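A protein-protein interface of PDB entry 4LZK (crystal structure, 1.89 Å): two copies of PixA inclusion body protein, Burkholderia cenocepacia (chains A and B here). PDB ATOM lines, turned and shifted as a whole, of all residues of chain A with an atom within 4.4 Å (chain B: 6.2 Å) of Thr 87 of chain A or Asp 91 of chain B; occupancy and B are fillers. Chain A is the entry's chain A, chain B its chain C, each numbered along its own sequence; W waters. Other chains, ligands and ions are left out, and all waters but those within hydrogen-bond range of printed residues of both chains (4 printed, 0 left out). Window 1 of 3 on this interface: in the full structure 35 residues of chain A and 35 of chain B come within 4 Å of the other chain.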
ATOM      1  N   LEU A  23     -10.496 -26.366  21.348  1.00  0.00           N
ATOM      2  CA  LEU A  23      -9.138 -26.840  21.404  1.00  0.00           C
ATOM      3  C   LEU A  23      -8.737 -26.978  22.857  1.00  0.00           C
ATOM      4  O   LEU A  23      -8.862 -26.006  23.626  1.00  0.00           O
ATOM      5  CB  LEU A  23      -8.198 -25.923  20.696  1.00  0.00           C
ATOM      6  CG  LEU A  23      -6.777 -26.455  20.674  1.00  0.00           C
ATOM      7  CD1 LEU A  23      -6.706 -27.751  19.801  1.00  0.00           C
ATOM      8  CD2 LEU A  23      -5.810 -25.459  20.153  1.00  0.00           C
ATOM      9  N   ALA A  24      -8.348 -28.138  23.243  1.00  0.00           N
ATOM     10  CA  ALA A  24      -7.805 -28.363  24.559  1.00  0.00           C
ATOM     11  C   ALA A  24      -6.282 -28.333  24.473  1.00  0.00           C
ATOM     12  O   ALA A  24      -5.672 -29.027  23.628  1.00  0.00           O
ATOM     13  CB  ALA A  24      -8.307 -29.678  25.075  1.00  0.00           C
ATOM     14  N   VAL A  25      -5.639 -27.457  25.248  1.00  0.00           N
ATOM     15  CA  VAL A  25      -4.221 -27.303  25.246  1.00  0.00           C
ATOM     16  C   VAL A  25      -3.694 -27.770  26.616  1.00  0.00           C
ATOM     17  O   VAL A  25      -4.021 -27.196  27.672  1.00  0.00           O
ATOM     18  CB  VAL A  25      -3.830 -25.857  24.981  1.00  0.00           C
ATOM     19  CG1 VAL A  25      -2.343 -25.607  25.054  1.00  0.00           C
ATOM     20  CG2 VAL A  25      -4.339 -25.435  23.621  1.00  0.00           C
ATOM     21  N   ILE A  26      -2.909 -28.838  26.563  1.00  0.00           N
ATOM     22  CA  ILE A  26      -2.510 -29.607  27.719  1.00  0.00           C
ATOM     23  C   ILE A  26      -1.071 -29.291  28.154  1.00  0.00           C
ATOM     24  O   ILE A  26      -0.141 -29.335  27.353  1.00  0.00           O
ATOM     25  CB  ILE A  26      -2.683 -31.069  27.352  1.00  0.00           C
ATOM     26  CG1 ILE A  26      -4.194 -31.286  27.096  1.00  0.00           C
ATOM     27  CG2 ILE A  26      -2.114 -31.930  28.434  1.00  0.00           C
ATOM     28  CD1 ILE A  26      -4.515 -32.609  26.575  1.00  0.00           C
ATOM     29  N   MET A  85     -10.516 -30.946  19.585  1.00  0.00           N
ATOM     30  CA  MET A  85      -9.146 -31.447  19.303  1.00  0.00           C
ATOM     31  C   MET A  85      -8.241 -31.143  20.467  1.00  0.00           C
ATOM     32  O   MET A  85      -8.585 -30.302  21.332  1.00  0.00           O
ATOM     33  CB  MET A  85      -8.585 -30.777  18.063  1.00  0.00           C
ATOM     34  CG  MET A  85      -9.541 -30.927  16.896  1.00  0.00           C
ATOM     35  SD  MET A  85      -8.715 -30.337  15.265  1.00  0.00           S
ATOM     36  CE  MET A  85      -7.010 -31.273  15.215  1.00  0.00           C
ATOM     37  N   GLY A  86      -7.106 -31.809  20.532  1.00  0.00           N
ATOM     38  CA  GLY A  86      -6.216 -31.625  21.641  1.00  0.00           C
ATOM     39  C   GLY A  86      -4.780 -31.593  21.200  1.00  0.00           C
ATOM     40  O   GLY A  86      -4.413 -32.198  20.161  1.00  0.00           O
ATOM     41  N   THR A  87      -3.980 -30.843  21.945  1.00  0.00           N
ATOM     42  CA  THR A  87      -2.591 -30.693  21.640  1.00  0.00           C
ATOM     43  C   THR A  87      -1.856 -30.200  22.855  1.00  0.00           C
ATOM     44  O   THR A  87      -2.491 -29.886  23.836  1.00  0.00           O
ATOM     45  CB  THR A  87      -2.385 -29.770  20.451  1.00  0.00           C
ATOM     46  OG1 THR A  87      -0.999 -29.862  20.025  1.00  0.00           O
ATOM     47  CG2 THR A  87      -2.738 -28.270  20.902  1.00  0.00           C
ATOM     48  N   SER A  88      -0.514 -30.137  22.814  1.00  0.00           N
ATOM     49  CA  SER A  88       0.290 -29.685  23.981  1.00  0.00           C
ATOM     50  C   SER A  88       0.589 -28.201  23.811  1.00  0.00           C
ATOM     51  O   SER A  88       0.309 -27.640  22.748  1.00  0.00           O
ATOM     52  CB  SER A  88       1.610 -30.454  24.024  1.00  0.00           C
ATOM     53  OG  SER A  88       2.444 -30.151  22.943  1.00  0.00           O
ATOM     54  N   ASP A  91       2.372 -27.651  20.847  1.00  0.00           N
ATOM     55  CA  ASP A  91       1.643 -28.080  19.666  1.00  0.00           C
ATOM     56  C   ASP A  91       1.979 -29.512  19.225  1.00  0.00           C
ATOM     57  O   ASP A  91       2.022 -29.785  18.001  1.00  0.00           O
ATOM     58  CB  ASP A  91       1.825 -27.149  18.476  1.00  0.00           C
ATOM     59  CG  ASP A  91       0.655 -27.214  17.528  1.00  0.00           C
ATOM     60  OD1 ASP A  91      -0.433 -27.746  17.985  1.00  0.00           O
ATOM     61  OD2 ASP A  91       0.775 -26.813  16.334  1.00  0.00           O
ATOM     62  N   ASN A  92       2.229 -30.361  20.205  1.00  0.00           N
ATOM     63  CA  ASN A  92       2.518 -31.790  19.939  1.00  0.00           C
ATOM     64  C   ASN A  92       3.813 -31.997  19.125  1.00  0.00           C
ATOM     65  O   ASN A  92       3.991 -33.030  18.493  1.00  0.00           O
ATOM     66  CB  ASN A  92       1.328 -32.560  19.348  1.00  0.00           C
ATOM     67  CG  ASN A  92       0.267 -32.876  20.345  1.00  0.00           C
ATOM     68  OD1 ASN A  92       0.429 -32.707  21.580  1.00  0.00           O
ATOM     69  ND2 ASN A  92      -0.841 -33.439  19.846  1.00  0.00           N
ATOM     70  N   ALA A  97       0.051 -34.776  23.251  1.00  0.00           N
ATOM     71  CA  ALA A  97      -1.198 -35.126  23.911  1.00  0.00           C
ATOM     72  C   ALA A  97      -2.211 -35.433  22.841  1.00  0.00           C
ATOM     73  O   ALA A  97      -2.520 -34.572  22.042  1.00  0.00           O
ATOM     74  CB  ALA A  97      -1.628 -33.938  24.787  1.00  0.00           C
ATOM     75  N   PHE A 143      -4.609 -35.786  11.572  1.00  0.00           N
ATOM     76  CA  PHE A 143      -5.199 -35.260  12.782  1.00  0.00           C
ATOM     77  C   PHE A 143      -6.510 -35.955  13.015  1.00  0.00           C
ATOM     78  O   PHE A 143      -7.149 -36.533  12.113  1.00  0.00           O
ATOM     79  CB  PHE A 143      -5.501 -33.720  12.633  1.00  0.00           C
ATOM     80  CG  PHE A 143      -4.341 -32.835  12.365  1.00  0.00           C
ATOM     81  CD1 PHE A 143      -3.901 -32.611  11.091  1.00  0.00           C
ATOM     82  CD2 PHE A 143      -3.737 -32.132  13.400  1.00  0.00           C
ATOM     83  CE1 PHE A 143      -2.901 -31.722  10.827  1.00  0.00           C
ATOM     84  CE2 PHE A 143      -2.712 -31.227  13.166  1.00  0.00           C
ATOM     85  CZ  PHE A 143      -2.301 -31.005  11.878  1.00  0.00           C
ATOM     86  N   LEU B  23       1.779 -20.771  23.600  1.00  0.00           N
ATOM     87  CA  LEU B  23       0.990 -21.125  22.437  1.00  0.00           C
ATOM     88  C   LEU B  23      -0.023 -20.046  22.128  1.00  0.00           C
ATOM     89  O   LEU B  23      -0.922 -19.693  22.962  1.00  0.00           O
ATOM     90  CB  LEU B  23       0.341 -22.521  22.586  1.00  0.00           C
ATOM     91  CG  LEU B  23      -0.323 -23.080  21.317  1.00  0.00           C
ATOM     92  CD1 LEU B  23       0.734 -23.383  20.257  1.00  0.00           C
ATOM     93  CD2 LEU B  23      -1.151 -24.296  21.694  1.00  0.00           C
ATOM     94  N   THR B  87      -1.070 -21.610  16.286  1.00  0.00           N
ATOM     95  CA  THR B  87      -1.870 -22.568  15.592  1.00  0.00           C
ATOM     96  C   THR B  87      -3.310 -22.121  15.571  1.00  0.00           C
ATOM     97  O   THR B  87      -3.683 -21.171  16.258  1.00  0.00           O
ATOM     98  CB  THR B  87      -1.770 -23.941  16.291  1.00  0.00           C
ATOM     99  OG1 THR B  87      -2.302 -24.972  15.421  1.00  0.00           O
ATOM    100  CG2 THR B  87      -2.507 -23.974  17.688  1.00  0.00           C
ATOM    101  N   SER B  88      -4.174 -22.822  14.833  1.00  0.00           N
ATOM    102  CA  SER B  88      -5.564 -22.395  14.816  1.00  0.00           C
ATOM    103  C   SER B  88      -6.349 -23.171  15.848  1.00  0.00           C
ATOM    104  O   SER B  88      -5.794 -24.087  16.550  1.00  0.00           O
ATOM    105  CB  SER B  88      -6.069 -22.608  13.368  1.00  0.00           C
ATOM    106  OG  SER B  88      -6.326 -24.006  13.237  1.00  0.00           O
ATOM    107  N   LEU B  89      -7.633 -22.885  15.918  1.00  0.00           N
ATOM    108  CA  LEU B  89      -8.547 -23.583  16.794  1.00  0.00           C
ATOM    109  C   LEU B  89      -8.733 -25.037  16.371  1.00  0.00           C
ATOM    110  O   LEU B  89      -9.106 -25.877  17.203  1.00  0.00           O
ATOM    111  CB  LEU B  89      -9.905 -22.877  16.905  1.00  0.00           C
ATOM    112  CG  LEU B  89      -9.924 -21.657  17.850  1.00  0.00           C
ATOM    113  CD1 LEU B  89     -11.121 -20.743  17.558  1.00  0.00           C
ATOM    114  CD2 LEU B  89      -9.945 -22.223  19.310  1.00  0.00           C
ATOM    115  N   ALA B  90      -8.466 -25.335  15.103  1.00  0.00           N
ATOM    116  CA  ALA B  90      -8.413 -26.736  14.702  1.00  0.00           C
ATOM    117  C   ALA B  90      -7.011 -27.195  14.485  1.00  0.00           C
ATOM    118  O   ALA B  90      -6.735 -28.033  13.632  1.00  0.00           O
ATOM    119  CB  ALA B  90      -9.301 -27.022  13.516  1.00  0.00           C
ATOM    120  N   ASP B  91      -6.098 -26.626  15.267  1.00  0.00           N
ATOM    121  CA  ASP B  91      -4.699 -27.048  15.310  1.00  0.00           C
ATOM    122  C   ASP B  91      -4.008 -27.082  13.969  1.00  0.00           C
ATOM    123  O   ASP B  91      -3.190 -27.993  13.696  1.00  0.00           O
ATOM    124  CB  ASP B  91      -4.553 -28.404  16.023  1.00  0.00           C
ATOM    125  CG  ASP B  91      -3.155 -28.599  16.565  1.00  0.00           C
ATOM    126  OD1 ASP B  91      -2.451 -27.572  16.751  1.00  0.00           O
ATOM    127  OD2 ASP B  91      -2.742 -29.739  16.815  1.00  0.00           O
ATOM    128  N   ASN B  92      -4.323 -26.090  13.119  1.00  0.00           N
ATOM    129  CA  ASN B  92      -3.732 -25.996  11.754  1.00  0.00           C
ATOM    130  C   ASN B  92      -4.019 -27.224  10.884  1.00  0.00           C
ATOM    131  O   ASN B  92      -3.258 -27.512   9.934  1.00  0.00           O
ATOM    132  CB  ASN B  92      -2.237 -25.732  11.810  1.00  0.00           C
ATOM    133  CG  ASN B  92      -1.920 -24.291  12.173  1.00  0.00           C
ATOM    134  OD1 ASN B  92      -2.796 -23.478  12.371  1.00  0.00           O
ATOM    135  ND2 ASN B  92      -0.637 -23.986  12.308  1.00  0.00           N
ATOM    136  N   SER B  93      -5.108 -27.898  11.169  1.00  0.00           N
ATOM    137  CA  SER B  93      -5.534 -29.087  10.368  1.00  0.00           C
ATOM    138  C   SER B  93      -6.302 -28.666   9.067  1.00  0.00           C
ATOM    139  O   SER B  93      -6.406 -29.423   8.163  1.00  0.00           O
ATOM    140  CB  SER B  93      -6.393 -30.018  11.208  1.00  0.00           C
ATOM    141  OG  SER B  93      -7.612 -29.436  11.544  1.00  0.00           O
ATOM    142  N   GLY B  94      -6.856 -27.477   9.054  1.00  0.00           N
ATOM    143  CA  GLY B  94      -7.636 -26.928   7.934  1.00  0.00           C
ATOM    144  C   GLY B  94      -7.044 -25.597   7.527  1.00  0.00           C
ATOM    145  O   GLY B  94      -5.984 -25.579   6.853  1.00  0.00           O
ATOM    146  N   ASP B  95      -7.631 -24.498   7.980  1.00  0.00           N
ATOM    147  CA  ASP B  95      -6.901 -23.216   7.902  1.00  0.00           C
ATOM    148  C   ASP B  95      -5.635 -23.430   8.750  1.00  0.00           C
ATOM    149  O   ASP B  95      -5.639 -24.251   9.674  1.00  0.00           O
ATOM    150  CB  ASP B  95      -7.643 -22.034   8.537  1.00  0.00           C
ATOM    151  CG  ASP B  95      -9.089 -21.815   8.026  1.00  0.00           C
ATOM    152  OD1 ASP B  95      -9.352 -22.035   6.824  1.00  0.00           O
ATOM    153  OD2 ASP B  95      -9.949 -21.325   8.863  1.00  0.00           O
ATOM    154  N   GLN B 141       4.888 -33.798  10.540  1.00  0.00           N
ATOM    155  CA  GLN B 141       4.859 -32.351  10.419  1.00  0.00           C
ATOM    156  C   GLN B 141       6.241 -31.730  10.684  1.00  0.00           C
ATOM    157  O   GLN B 141       6.990 -32.235  11.485  1.00  0.00           O
ATOM    158  CB  GLN B 141       3.866 -31.811  11.434  1.00  0.00           C
ATOM    159  CG  GLN B 141       2.590 -31.194  10.910  1.00  0.00           C
ATOM    160  CD  GLN B 141       2.324 -29.912  11.672  1.00  0.00           C
ATOM    161  OE1 GLN B 141       3.254 -29.356  12.244  1.00  0.00           O
ATOM    162  NE2 GLN B 141       1.076 -29.433  11.694  1.00  0.00           N
HETATM  163  O   HOH W   1     -10.956 -27.944  17.183  1.00  0.00           O
HETATM  164  O   HOH W   2      -0.404 -28.240  14.169  1.00  0.00           O
HETATM  165  O   HOH W   3      -4.218 -31.980  17.493  1.00  0.00           O
HETATM  166  O   HOH W   4      -0.235 -30.544  16.282  1.00  0.00           O
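Water W3 bridges the backbone carbonyl oxygen (O) of Gly 86 of chain A and the side-chain carboxylate (OD2) of Asp 91 of chain B.
Water W4 lies within hydrogen-bond range of the side-chain carboxylate (OD2) of Asp 91 of chain B and the backbone carbonyl oxygen (O) of Asp 91 of chain A.
Water W1 lies within hydrogen-bond range of the backbone carbonyl oxygen (O) of Leu 89 of chain B (2.8 Å) and the side-chain sulfur (SD) of Met 85 of chain A (3.8 Å).
Water W2 lies within hydrogen-bond range of the backbone carbonyl oxygen (O) of Asp 91 of chain B (2.8 Å), the side-chain carboxylate (OD2) of Asp 91 of chain A (2.8 Å) and the side-chain amide nitrogen (NE2) of Gln 141 of chain B (3.1 Å).
Leu 23 of chain A touches Ser 88 of chain B, and with the chains exchanged Ser 88 of chain A touches Leu 23 of chain B.
Thr 87 of chain A touches Asp 91 of chain B, and with the chains exchanged Asp 91 of chain A touches Thr 87 of chain B.
Asp 91 of chain A touches its own counterpart, Asp 91 of chain B.
Printed residues of chain A that touch a printed residue of chain B: Leu 23, Val 25, Met 85, Thr 87, Ser 88, Asp 91 and Phe 143.
Hydrophobic or aromatic side chains of chain A within 4 Å of the printed part of chain B: Leu 23, Val 25, Met 85 and Phe 143.
Of the 11 printed residues of chain B, 8 touch a printed residue of chain A.
Printed residues of chain B that touch a printed residue of chain A: Leu 23, Thr 87, Ser 88, Leu 89, Ala 90, Asp 91, Ser 93 and Gln 141.
Hydrophobic or aromatic side chains of chain B that line the printed part of chain A: Leu 23 and Ala 90.
Among the printed residues, no Asp or Glu carboxylate lies within 4 Å of a Lys or Arg side-chain nitrogen of the other chain.
SD of Met 85 of chain A sits close to O of Ala 90 of chain B.
OD1 of Asp 91 of chain B sits close to OD1 of Asp 91 of chain A.
The backbone NH of Thr 87 of chain A sits at hydrogen-bond distance from the backbone carbonyl oxygen of Ala 24 of chain A (3.0 Å).
N of Ile 26 of chain A is in hydrogen-bond range of O of Thr 87 of chain A, 3.0 Å away.
OG of Ser 88 of chain A lies within hydrogen-bond range of N of Asn 92 of chain A, at 2.8 Å.
The side-chain hydroxyl (OG) of Ser 88 of chain B sits close to the backbone NH (N) of Ala 90 of chain B (3.1 Å).
The backbone NH of Asn 92 of chain B sits at hydrogen-bond distance from the side-chain hydroxyl of Ser 88 of chain B, 2.9 Å away.
The backbone carbonyl oxygen (O) of Ala 90 of chain B sits at hydrogen-bond distance from the side-chain hydroxyl (OG) of Ser 93 of chain B.
Of the printed residues of chain B, Met 85 of chain A touches Ala 90, Asp 91 and Ser 93.
Thr 87 of chain A touches one residue of chain B.
Printed residues of chain B within 4 Å of Asp 91 of chain A: Thr 87 (3.7 Å) and Asp 91 (2.4 Å).
Printed residues of chain A within 4 Å of Asp 91 of chain B: Met 85 (3.9 Å), Thr 87 (3.7 Å), Asp 91 (2.4 Å) and Phe 143 (3.3 Å).
Asp 95 of chain B touches none of the printed residues of chain A.
The nearest printed residue of chain A that does not touch Asp 91 of chain B is Leu 23 of chain A (4.4 Å).
The nearest printed residue of chain B that does not touch Met 85 of chain A is Leu 89 of chain B (4.9 Å).
Leu 23 of chain A touches Ser 88 of chain B.
CB of Leu 23 of chain A touches O of Leu 89 of chain B, 3.6 Å away.
CG1 of Val 25 of chain A touches CD2 of Leu 23 of chain B (3.8 Å).
Asp 91 of chain B touches Met 85 of chain A (CB to CE, 3.9 Å).
Ser 93 of chain B touches Met 85 of chain A.
Ser 88 of chain A touches Leu 23 of chain B (O to CD2, 3.8 Å).
OG1 of Thr 87 of chain B touches OD2 of Asp 91 of chain A, 3.7 Å away.
Asp 91 of chain B touches Phe 143 of chain A.
Ser 93 of chain B touches Phe 143 of chain A (CB to CD1, 3.6 Å).
CZ of Phe 143 of chain A touches NE2 of Gln 141 of chain B (3.7 Å).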
